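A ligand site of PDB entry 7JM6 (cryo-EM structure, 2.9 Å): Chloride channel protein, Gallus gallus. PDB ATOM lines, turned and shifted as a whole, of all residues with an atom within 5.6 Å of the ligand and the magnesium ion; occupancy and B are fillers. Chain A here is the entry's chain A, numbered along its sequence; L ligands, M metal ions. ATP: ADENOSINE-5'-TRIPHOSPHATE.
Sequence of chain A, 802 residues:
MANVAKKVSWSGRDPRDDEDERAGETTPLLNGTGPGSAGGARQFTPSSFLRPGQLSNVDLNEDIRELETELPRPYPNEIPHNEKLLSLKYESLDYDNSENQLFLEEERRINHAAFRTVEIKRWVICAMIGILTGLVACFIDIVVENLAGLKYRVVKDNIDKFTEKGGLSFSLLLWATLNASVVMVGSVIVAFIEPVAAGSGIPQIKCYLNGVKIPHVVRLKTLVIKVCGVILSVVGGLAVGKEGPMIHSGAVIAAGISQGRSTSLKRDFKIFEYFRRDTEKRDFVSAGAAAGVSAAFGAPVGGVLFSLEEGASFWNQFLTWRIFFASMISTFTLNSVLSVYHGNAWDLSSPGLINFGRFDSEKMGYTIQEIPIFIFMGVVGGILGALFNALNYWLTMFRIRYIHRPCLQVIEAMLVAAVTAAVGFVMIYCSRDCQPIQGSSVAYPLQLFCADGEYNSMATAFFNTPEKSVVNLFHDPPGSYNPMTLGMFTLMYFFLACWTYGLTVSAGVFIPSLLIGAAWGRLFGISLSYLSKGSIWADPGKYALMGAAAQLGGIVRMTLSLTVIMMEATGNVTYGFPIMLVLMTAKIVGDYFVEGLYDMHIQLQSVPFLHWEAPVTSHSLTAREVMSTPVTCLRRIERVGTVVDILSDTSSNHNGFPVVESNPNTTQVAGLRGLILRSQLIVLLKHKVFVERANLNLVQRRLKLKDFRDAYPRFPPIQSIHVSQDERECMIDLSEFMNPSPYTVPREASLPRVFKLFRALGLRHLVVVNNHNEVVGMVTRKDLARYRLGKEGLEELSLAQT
The magnesium ion is bound by O1B of the ligand.
The magnesium ion has one donor atom within binding distance.
Slightly farther from the magnesium ion lies the side-chain carboxylate (OE1) of Glu 91 (2.6 Å).
Slightly farther from the magnesium ion lies an oxygen (O1G) of the ligand (2.7 Å).
Slightly farther from the magnesium ion lies an oxygen (O2A) of the ligand (2.8 Å).
Asn 655 touches the magnesium ion.
Along chain A the residues within 4 Å of the magnesium ion span positions 91 to 655.
The nearest printed residue that does not touch the magnesium ion is Tyr 90 (4.2 Å).
An oxygen (O1A) of the ligand sits close to the backbone carbonyl oxygen (O) of Asn 653, at 3.1 Å.
Tyr 90 touches the ligand.
Pro 630 touches the ligand.
Val 631 touches the ligand (CA to N1, 3.4 Å).
CD of Pro 658 touches N6 of the ligand, at 3.9 Å.
Met 778 touches the ligand (CE to N6, 3.8 Å).
Thr 780 touches the ligand.
Hydrophobic or aromatic side chains that line the ligand: Val 631, His 654, Pro 658 and Met 778.
Within 4 Å of the ligand: Tyr 90, Glu 91, Ser 92, Ser 628, Pro 630, Val 631, Thr 632, Asn 653, His 654, Asn 655, Gly 656, Pro 658, Arg 764, His 765, Met 778, Thr 780 and Asp 783.
The side-chain carboxylate (OD1) of Asp 783 sits at hydrogen-bond distance from the backbone NH (N) of Thr 780, 3.0 Å away.
O of Met 778 is in hydrogen-bond range of N of Ser 628, 2.9 Å away.
A ring nitrogen (NE2) of His 765 sits close to the backbone NH of Gly 656, 3.4 Å away.
NE2 of His 654 lies within hydrogen-bond range of OG of Ser 652.
OG of Ser 92 sits at hydrogen-bond distance from NE of Arg 781.
The side-chain amide nitrogen (ND2) of Asn 655 sits at hydrogen-bond distance from the side-chain carboxylate (OE1) of Glu 91, at 3.2 Å.
OD2 of Asp 783 is in salt-bridge range of NH2 of Arg 786, 2.7 Å away.
The side-chain hydroxyl (OG) of Ser 628 sits at hydrogen-bond distance from the side-chain carboxylate (OD1) of Asp 783, 3.3 Å away.
The side-chain amide nitrogen (ND2) of Asn 655 lies close to an oxygen (O1B) of the ligand, at 3.2 Å.
An oxygen (O2') of the ligand lies within hydrogen-bond range of the side-chain carboxylate of Asp 783 (2.9 Å).
NE of Arg 764 lies within salt-bridge range of O2G of the ligand (2.4 Å).
The backbone NH (N) of His 654 lies close to an oxygen (O1A) of the ligand, 3.4 Å away.
O of Gly 656 lies within hydrogen-bond range of N6 of the ligand, 3.2 Å away.
The side-chain hydroxyl (OG) of Ser 628 sits at hydrogen-bond distance from an oxygen (O2') of the ligand (2.5 Å).
The backbone carbonyl oxygen of Thr 632 sits at hydrogen-bond distance from a nitrogen (N6) of the ligand (3.3 Å).
N of Thr 632 lies within hydrogen-bond range of N1 of the ligand.
ND1 of His 654 sits at hydrogen-bond distance from O1A of the ligand (3.2 Å).
O3G of the ligand sits at hydrogen-bond distance from OG of Ser 92, 2.8 Å away.
A ring nitrogen (NE2) of His 765 lies within hydrogen-bond range of an oxygen (O2B) of the ligand (3.2 Å).
O2B of the ligand sits at hydrogen-bond distance from N of Asn 655, 3.3 Å away.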
ATOM      1  N   LEU A  88      11.150 -21.088  -7.096  1.00  0.00           N
ATOM      2  CA  LEU A  88      10.231 -21.163  -8.227  1.00  0.00           C
ATOM      3  C   LEU A  88      10.871 -20.768  -9.548  1.00  0.00           C
ATOM      4  O   LEU A  88      10.237 -20.907 -10.595  1.00  0.00           O
ATOM      5  CB  LEU A  88       9.006 -20.273  -7.959  1.00  0.00           C
ATOM      6  CG  LEU A  88       7.967 -20.832  -6.987  1.00  0.00           C
ATOM      7  CD1 LEU A  88       8.602 -21.341  -5.709  1.00  0.00           C
ATOM      8  CD2 LEU A  88       6.917 -19.762  -6.668  1.00  0.00           C
ATOM      9  N   TYR A  90      12.969 -22.362 -11.073  1.00  0.00           N
ATOM     10  CA  TYR A  90      13.290 -23.583 -11.792  1.00  0.00           C
ATOM     11  C   TYR A  90      12.020 -24.403 -12.021  1.00  0.00           C
ATOM     12  O   TYR A  90      11.296 -24.717 -11.074  1.00  0.00           O
ATOM     13  CB  TYR A  90      14.310 -24.413 -11.003  1.00  0.00           C
ATOM     14  CG  TYR A  90      15.487 -23.616 -10.501  1.00  0.00           C
ATOM     15  CD1 TYR A  90      16.502 -23.233 -11.355  1.00  0.00           C
ATOM     16  CD2 TYR A  90      15.568 -23.241  -9.167  1.00  0.00           C
ATOM     17  CE1 TYR A  90      17.575 -22.506 -10.902  1.00  0.00           C
ATOM     18  CE2 TYR A  90      16.643 -22.517  -8.705  1.00  0.00           C
ATOM     19  CZ  TYR A  90      17.651 -22.150  -9.573  1.00  0.00           C
ATOM     20  OH  TYR A  90      18.725 -21.422  -9.120  1.00  0.00           O
ATOM     21  N   GLU A  91      11.765 -24.737 -13.283  1.00  0.00           N
ATOM     22  CA  GLU A  91      10.674 -25.624 -13.646  1.00  0.00           C
ATOM     23  C   GLU A  91      11.195 -27.055 -13.730  1.00  0.00           C
ATOM     24  O   GLU A  91      12.313 -27.354 -13.288  1.00  0.00           O
ATOM     25  CB  GLU A  91      10.044 -25.159 -14.959  1.00  0.00           C
ATOM     26  CG  GLU A  91       9.797 -23.668 -15.047  1.00  0.00           C
ATOM     27  CD  GLU A  91       8.731 -23.188 -14.084  1.00  0.00           C
ATOM     28  OE1 GLU A  91       7.611 -23.723 -14.120  1.00  0.00           O
ATOM     29  OE2 GLU A  91       9.028 -22.277 -13.283  1.00  0.00           O
ATOM     30  N   SER A  92      10.400 -27.950 -14.300  1.00  0.00           N
ATOM     31  CA  SER A  92      10.740 -29.365 -14.373  1.00  0.00           C
ATOM     32  C   SER A  92      10.465 -29.902 -15.770  1.00  0.00           C
ATOM     33  O   SER A  92       9.645 -29.363 -16.512  1.00  0.00           O
ATOM     34  CB  SER A  92       9.968 -30.190 -13.346  1.00  0.00           C
ATOM     35  OG  SER A  92      10.296 -29.803 -12.026  1.00  0.00           O
ATOM     36  N   SER A 628      -0.215 -30.859  -1.399  1.00  0.00           N
ATOM     37  CA  SER A 628      -0.611 -29.461  -1.334  1.00  0.00           C
ATOM     38  C   SER A 628      -2.114 -29.344  -1.540  1.00  0.00           C
ATOM     39  O   SER A 628      -2.664 -29.912  -2.491  1.00  0.00           O
ATOM     40  CB  SER A 628       0.132 -28.640  -2.400  1.00  0.00           C
ATOM     41  OG  SER A 628       1.527 -28.637  -2.160  1.00  0.00           O
ATOM     42  N   PRO A 630      -5.591 -26.378  -0.971  1.00  0.00           N
ATOM     43  CA  PRO A 630      -6.539 -26.986  -1.914  1.00  0.00           C
ATOM     44  C   PRO A 630      -5.964 -27.063  -3.320  1.00  0.00           C
ATOM     45  O   PRO A 630      -4.990 -26.383  -3.608  1.00  0.00           O
ATOM     46  CB  PRO A 630      -7.738 -26.041  -1.866  1.00  0.00           C
ATOM     47  CG  PRO A 630      -7.150 -24.740  -1.518  1.00  0.00           C
ATOM     48  CD  PRO A 630      -6.049 -25.043  -0.555  1.00  0.00           C
ATOM     49  N   VAL A 631      -6.579 -27.873  -4.188  1.00  0.00           N
ATOM     50  CA  VAL A 631      -6.070 -28.109  -5.539  1.00  0.00           C
ATOM     51  C   VAL A 631      -6.933 -27.369  -6.550  1.00  0.00           C
ATOM     52  O   VAL A 631      -8.161 -27.358  -6.440  1.00  0.00           O
ATOM     53  CB  VAL A 631      -6.025 -29.625  -5.852  1.00  0.00           C
ATOM     54  CG1 VAL A 631      -5.267 -29.872  -7.138  1.00  0.00           C
ATOM     55  CG2 VAL A 631      -5.386 -30.369  -4.722  1.00  0.00           C
ATOM     56  N   THR A 632      -6.277 -26.744  -7.526  1.00  0.00           N
ATOM     57  CA  THR A 632      -6.957 -26.056  -8.614  1.00  0.00           C
ATOM     58  C   THR A 632      -7.159 -27.030  -9.756  1.00  0.00           C
ATOM     59  O   THR A 632      -6.194 -27.434 -10.415  1.00  0.00           O
ATOM     60  CB  THR A 632      -6.154 -24.838  -9.056  1.00  0.00           C
ATOM     61  OG1 THR A 632      -5.974 -23.942  -7.956  1.00  0.00           O
ATOM     62  CG2 THR A 632      -6.857 -24.112 -10.181  1.00  0.00           C
ATOM     63  N   CYS A 633      -8.412 -27.415 -10.000  1.00  0.00           N
ATOM     64  CA  CYS A 633      -8.744 -28.410 -11.002  1.00  0.00           C
ATOM     65  C   CYS A 633      -9.643 -27.814 -12.074  1.00  0.00           C
ATOM     66  O   CYS A 633     -10.287 -26.772 -11.870  1.00  0.00           O
ATOM     67  CB  CYS A 633      -9.433 -29.623 -10.364  1.00  0.00           C
ATOM     68  SG  CYS A 633      -8.505 -30.349  -8.998  1.00  0.00           S
ATOM     69  N   SER A 652      -0.092 -17.596  -8.470  1.00  0.00           N
ATOM     70  CA  SER A 652       0.573 -18.880  -8.626  1.00  0.00           C
ATOM     71  C   SER A 652       0.836 -19.120 -10.109  1.00  0.00           C
ATOM     72  O   SER A 652       0.211 -18.493 -10.981  1.00  0.00           O
ATOM     73  CB  SER A 652      -0.276 -20.027  -8.059  1.00  0.00           C
ATOM     74  OG  SER A 652      -1.530 -20.108  -8.705  1.00  0.00           O
ATOM     75  N   ASN A 653       1.776 -20.015 -10.398  1.00  0.00           N
ATOM     76  CA  ASN A 653       2.162 -20.348 -11.760  1.00  0.00           C
ATOM     77  C   ASN A 653       2.179 -21.871 -11.911  1.00  0.00           C
ATOM     78  O   ASN A 653       3.136 -22.467 -12.406  1.00  0.00           O
ATOM     79  CB  ASN A 653       3.524 -19.748 -12.112  1.00  0.00           C
ATOM     80  CG  ASN A 653       3.723 -19.610 -13.604  1.00  0.00           C
ATOM     81  OD1 ASN A 653       3.170 -18.713 -14.243  1.00  0.00           O
ATOM     82  ND2 ASN A 653       4.534 -20.492 -14.176  1.00  0.00           N
ATOM     83  N   HIS A 654       1.100 -22.507 -11.466  1.00  0.00           N
ATOM     84  CA  HIS A 654       0.975 -23.959 -11.605  1.00  0.00           C
ATOM     85  C   HIS A 654       0.989 -24.337 -13.082  1.00  0.00           C
ATOM     86  O   HIS A 654       0.342 -23.707 -13.907  1.00  0.00           O
ATOM     87  CB  HIS A 654      -0.305 -24.451 -10.946  1.00  0.00           C
ATOM     88  CG  HIS A 654      -0.494 -23.983  -9.541  1.00  0.00           C
ATOM     89  ND1 HIS A 654       0.497 -24.067  -8.587  1.00  0.00           N
ATOM     90  CD2 HIS A 654      -1.568 -23.439  -8.917  1.00  0.00           C
ATOM     91  CE1 HIS A 654       0.058 -23.586  -7.447  1.00  0.00           C
ATOM     92  NE2 HIS A 654      -1.196 -23.194  -7.617  1.00  0.00           N
ATOM     93  N   ASN A 655       1.728 -25.400 -13.403  1.00  0.00           N
ATOM     94  CA  ASN A 655       1.840 -25.896 -14.762  1.00  0.00           C
ATOM     95  C   ASN A 655       1.161 -27.236 -14.971  1.00  0.00           C
ATOM     96  O   ASN A 655       1.284 -27.822 -16.053  1.00  0.00           O
ATOM     97  CB  ASN A 655       3.321 -25.996 -15.172  1.00  0.00           C
ATOM     98  CG  ASN A 655       3.956 -24.645 -15.388  1.00  0.00           C
ATOM     99  OD1 ASN A 655       4.040 -24.157 -16.519  1.00  0.00           O
ATOM    100  ND2 ASN A 655       4.424 -24.039 -14.317  1.00  0.00           N
ATOM    101  N   GLY A 656       0.456 -27.752 -13.964  1.00  0.00           N
ATOM    102  CA  GLY A 656      -0.265 -28.996 -14.104  1.00  0.00           C
ATOM    103  C   GLY A 656      -1.569 -28.948 -13.345  1.00  0.00           C
ATOM    104  O   GLY A 656      -1.597 -28.589 -12.169  1.00  0.00           O
ATOM    105  N   PHE A 657      -2.668 -29.326 -14.003  1.00  0.00           N
ATOM    106  CA  PHE A 657      -3.991 -29.207 -13.442  1.00  0.00           C
ATOM    107  C   PHE A 657      -4.724 -30.538 -13.565  1.00  0.00           C
ATOM    108  O   PHE A 657      -4.858 -31.067 -14.685  1.00  0.00           O
ATOM    109  CB  PHE A 657      -4.772 -28.102 -14.150  1.00  0.00           C
ATOM    110  CG  PHE A 657      -4.054 -26.798 -14.224  1.00  0.00           C
ATOM    111  CD1 PHE A 657      -4.164 -25.868 -13.206  1.00  0.00           C
ATOM    112  CD2 PHE A 657      -3.234 -26.502 -15.297  1.00  0.00           C
ATOM    113  CE1 PHE A 657      -3.492 -24.675 -13.264  1.00  0.00           C
ATOM    114  CE2 PHE A 657      -2.553 -25.310 -15.358  1.00  0.00           C
ATOM    115  CZ  PHE A 657      -2.686 -24.396 -14.341  1.00  0.00           C
ATOM    116  N   PRO A 658      -5.191 -31.112 -12.465  1.00  0.00           N
ATOM    117  CA  PRO A 658      -6.060 -32.289 -12.572  1.00  0.00           C
ATOM    118  C   PRO A 658      -7.382 -31.935 -13.240  1.00  0.00           C
ATOM    119  O   PRO A 658      -7.909 -30.835 -13.068  1.00  0.00           O
ATOM    120  CB  PRO A 658      -6.265 -32.723 -11.118  1.00  0.00           C
ATOM    121  CG  PRO A 658      -5.161 -32.065 -10.363  1.00  0.00           C
ATOM    122  CD  PRO A 658      -4.926 -30.778 -11.056  1.00  0.00           C
ATOM    123  N   ARG A 764       6.339 -35.323 -12.971  1.00  0.00           N
ATOM    124  CA  ARG A 764       6.268 -33.912 -12.645  1.00  0.00           C
ATOM    125  C   ARG A 764       5.117 -33.596 -11.710  1.00  0.00           C
ATOM    126  O   ARG A 764       5.235 -32.688 -10.872  1.00  0.00           O
ATOM    127  CB  ARG A 764       6.131 -33.080 -13.920  1.00  0.00           C
ATOM    128  CG  ARG A 764       6.305 -31.591 -13.724  1.00  0.00           C
ATOM    129  CD  ARG A 764       6.147 -30.853 -15.026  1.00  0.00           C
ATOM    130  NE  ARG A 764       6.440 -29.437 -14.893  1.00  0.00           N
ATOM    131  CZ  ARG A 764       6.173 -28.526 -15.815  1.00  0.00           C
ATOM    132  NH1 ARG A 764       6.478 -27.262 -15.604  1.00  0.00           N
ATOM    133  NH2 ARG A 764       5.596 -28.884 -16.961  1.00  0.00           N
ATOM    134  N   HIS A 765       4.021 -34.329 -11.822  1.00  0.00           N
ATOM    135  CA  HIS A 765       2.849 -34.152 -10.981  1.00  0.00           C
ATOM    136  C   HIS A 765       2.361 -35.504 -10.502  1.00  0.00           C
ATOM    137  O   HIS A 765       2.341 -36.475 -11.270  1.00  0.00           O
ATOM    138  CB  HIS A 765       1.724 -33.435 -11.736  1.00  0.00           C
ATOM    139  CG  HIS A 765       2.150 -32.146 -12.362  1.00  0.00           C
ATOM    140  ND1 HIS A 765       2.437 -32.037 -13.708  1.00  0.00           N
ATOM    141  CD2 HIS A 765       2.328 -30.920 -11.836  1.00  0.00           C
ATOM    142  CE1 HIS A 765       2.786 -30.787 -13.974  1.00  0.00           C
ATOM    143  NE2 HIS A 765       2.729 -30.085 -12.866  1.00  0.00           N
ATOM    144  N   MET A 778      -1.996 -32.486  -4.345  1.00  0.00           N
ATOM    145  CA  MET A 778      -1.008 -32.558  -5.411  1.00  0.00           C
ATOM    146  C   MET A 778       0.383 -32.631  -4.781  1.00  0.00           C
ATOM    147  O   MET A 778       0.726 -31.793  -3.947  1.00  0.00           O
ATOM    148  CB  MET A 778      -1.117 -31.361  -6.343  1.00  0.00           C
ATOM    149  CG  MET A 778      -0.064 -31.311  -7.444  1.00  0.00           C
ATOM    150  SD  MET A 778      -0.495 -32.343  -8.845  1.00  0.00           S
ATOM    151  CE  MET A 778      -1.392 -31.157  -9.828  1.00  0.00           C
ATOM    152  N   VAL A 779       1.168 -33.614  -5.200  1.00  0.00           N
ATOM    153  CA  VAL A 779       2.552 -33.760  -4.794  1.00  0.00           C
ATOM    154  C   VAL A 779       3.436 -33.474  -5.997  1.00  0.00           C
ATOM    155  O   VAL A 779       3.249 -34.066  -7.075  1.00  0.00           O
ATOM    156  CB  VAL A 779       2.827 -35.166  -4.239  1.00  0.00           C
ATOM    157  CG1 VAL A 779       4.312 -35.384  -4.040  1.00  0.00           C
ATOM    158  CG2 VAL A 779       2.080 -35.372  -2.938  1.00  0.00           C
ATOM    159  N   THR A 780       4.378 -32.564  -5.826  1.00  0.00           N
ATOM    160  CA  THR A 780       5.332 -32.191  -6.864  1.00  0.00           C
ATOM    161  C   THR A 780       6.751 -32.350  -6.329  1.00  0.00           C
ATOM    162  O   THR A 780       6.983 -32.876  -5.238  1.00  0.00           O
ATOM    163  CB  THR A 780       5.095 -30.760  -7.353  1.00  0.00           C
ATOM    164  OG1 THR A 780       5.502 -29.827  -6.340  1.00  0.00           O
ATOM    165  CG2 THR A 780       3.637 -30.533  -7.681  1.00  0.00           C
ATOM    166  N   ARG A 781       7.723 -31.943  -7.158  1.00  0.00           N
ATOM    167  CA  ARG A 781       9.161 -32.014  -6.800  1.00  0.00           C
ATOM    168  C   ARG A 781       9.451 -31.233  -5.530  1.00  0.00           C
ATOM    169  O   ARG A 781      10.221 -31.752  -4.743  1.00  0.00           O
ATOM    170  CB  ARG A 781       9.966 -31.445  -7.965  1.00  0.00           C
ATOM    171  CG  ARG A 781      11.470 -31.413  -7.723  1.00  0.00           C
ATOM    172  CD  ARG A 781      12.152 -30.922  -8.967  1.00  0.00           C
ATOM    173  NE  ARG A 781      12.057 -31.897 -10.042  1.00  0.00           N
ATOM    174  CZ  ARG A 781      12.790 -32.991 -10.171  1.00  0.00           C
ATOM    175  NH1 ARG A 781      13.747 -33.298  -9.303  1.00  0.00           N
ATOM    176  NH2 ARG A 781      12.567 -33.803 -11.196  1.00  0.00           N
ATOM    177  N   LYS A 782       8.924 -30.005  -5.360  1.00  0.00           N
ATOM    178  CA  LYS A 782       9.220 -29.200  -4.179  1.00  0.00           C
ATOM    179  C   LYS A 782       8.583 -29.798  -2.933  1.00  0.00           C
ATOM    180  O   LYS A 782       9.075 -29.591  -1.821  1.00  0.00           O
ATOM    181  CB  LYS A 782       8.736 -27.775  -4.409  1.00  0.00           C
ATOM    182  CG  LYS A 782       9.483 -27.072  -5.513  1.00  0.00           C
ATOM    183  CD  LYS A 782       9.005 -25.646  -5.712  1.00  0.00           C
ATOM    184  CE  LYS A 782       9.727 -25.015  -6.877  1.00  0.00           C
ATOM    185  NZ  LYS A 782      11.165 -24.875  -6.590  1.00  0.00           N
ATOM    186  N   ASP A 783       7.485 -30.524  -3.106  1.00  0.00           N
ATOM    187  CA  ASP A 783       6.848 -31.178  -1.962  1.00  0.00           C
ATOM    188  C   ASP A 783       7.737 -32.244  -1.364  1.00  0.00           C
ATOM    189  O   ASP A 783       7.762 -32.430  -0.145  1.00  0.00           O
ATOM    190  CB  ASP A 783       5.504 -31.769  -2.383  1.00  0.00           C
ATOM    191  CG  ASP A 783       4.520 -30.725  -2.824  1.00  0.00           C
ATOM    192  OD1 ASP A 783       3.450 -31.094  -3.346  1.00  0.00           O
ATOM    193  OD2 ASP A 783       4.810 -29.527  -2.632  1.00  0.00           O
ATOM    194  N   ARG A 786      11.390 -30.793   0.175  1.00  0.00           N
ATOM    195  CA  ARG A 786      11.383 -29.969   1.378  1.00  0.00           C
ATOM    196  C   ARG A 786      11.961 -30.729   2.575  1.00  0.00           C
ATOM    197  O   ARG A 786      12.718 -30.154   3.369  1.00  0.00           O
ATOM    198  CB  ARG A 786       9.977 -29.476   1.687  1.00  0.00           C
ATOM    199  CG  ARG A 786       9.005 -30.566   2.111  1.00  0.00           C
ATOM    200  CD  ARG A 786       7.593 -30.029   2.308  1.00  0.00           C
ATOM    201  NE  ARG A 786       6.969 -29.604   1.056  1.00  0.00           N
ATOM    202  CZ  ARG A 786       5.798 -28.973   0.990  1.00  0.00           C
ATOM    203  NH1 ARG A 786       5.119 -28.703   2.091  1.00  0.00           N
ATOM    204  NH2 ARG A 786       5.304 -28.609  -0.186  1.00  0.00           N
HETATM  205  PG  ATP L   1       7.459 -27.969 -11.455  1.00  0.00           P
HETATM  206  O1G ATP L   1       7.977 -26.616 -11.885  1.00  0.00           O
HETATM  207  O2G ATP L   1       7.015 -28.860 -12.587  1.00  0.00           O
HETATM  208  O3G ATP L   1       8.309 -28.653 -10.403  1.00  0.00           O
HETATM  209  PB  ATP L   1       5.057 -26.553 -11.252  1.00  0.00           P
HETATM  210  O1B ATP L   1       5.806 -25.319 -11.670  1.00  0.00           O
HETATM  211  O2B ATP L   1       4.122 -27.260 -12.197  1.00  0.00           O
HETATM  212  O3B ATP L   1       6.103 -27.638 -10.674  1.00  0.00           O
HETATM  213  PA  ATP L   1       4.509 -24.861  -9.111  1.00  0.00           P
HETATM  214  O1A ATP L   1       3.571 -23.794  -9.595  1.00  0.00           O
HETATM  215  O2A ATP L   1       5.996 -24.622  -9.066  1.00  0.00           O
HETATM  216  O3A ATP L   1       4.240 -26.221  -9.919  1.00  0.00           O
HETATM  217  O5' ATP L   1       4.050 -25.335  -7.652  1.00  0.00           O
HETATM  218  C5' ATP L   1       4.297 -24.558  -6.483  1.00  0.00           C
HETATM  219  C4' ATP L   1       3.526 -25.238  -5.368  1.00  0.00           C
HETATM  220  O4' ATP L   1       2.152 -25.300  -5.757  1.00  0.00           O
HETATM  221  C3' ATP L   1       4.020 -26.653  -5.147  1.00  0.00           C
HETATM  222  O3' ATP L   1       4.461 -26.810  -3.792  1.00  0.00           O
HETATM  223  C2' ATP L   1       2.853 -27.557  -5.461  1.00  0.00           C
HETATM  224  O2' ATP L   1       2.618 -28.514  -4.431  1.00  0.00           O
HETATM  225  C1' ATP L   1       1.651 -26.631  -5.609  1.00  0.00           C
HETATM  226  N9  ATP L   1       0.784 -26.987  -6.761  1.00  0.00           N
HETATM  227  C8  ATP L   1       1.154 -27.382  -8.002  1.00  0.00           C
HETATM  228  N7  ATP L   1       0.068 -27.604  -8.772  1.00  0.00           N
HETATM  229  C5  ATP L   1      -1.029 -27.355  -8.025  1.00  0.00           C
HETATM  230  C6  ATP L   1      -2.491 -27.390  -8.211  1.00  0.00           C
HETATM  231  N6  ATP L   1      -3.033 -27.746  -9.393  1.00  0.00           N
HETATM  232  N1  ATP L   1      -3.261 -27.041  -7.166  1.00  0.00           N
HETATM  233  C2  ATP L   1      -2.738 -26.682  -5.980  1.00  0.00           C
HETATM  234  N3  ATP L   1      -1.418 -26.629  -5.745  1.00  0.00           N
HETATM  235  C4  ATP L   1      -0.534 -26.949  -6.714  1.00  0.00           C
HETATM  236 MG    MG M   1       7.206 -24.009 -11.551  1.00  0.00          MG
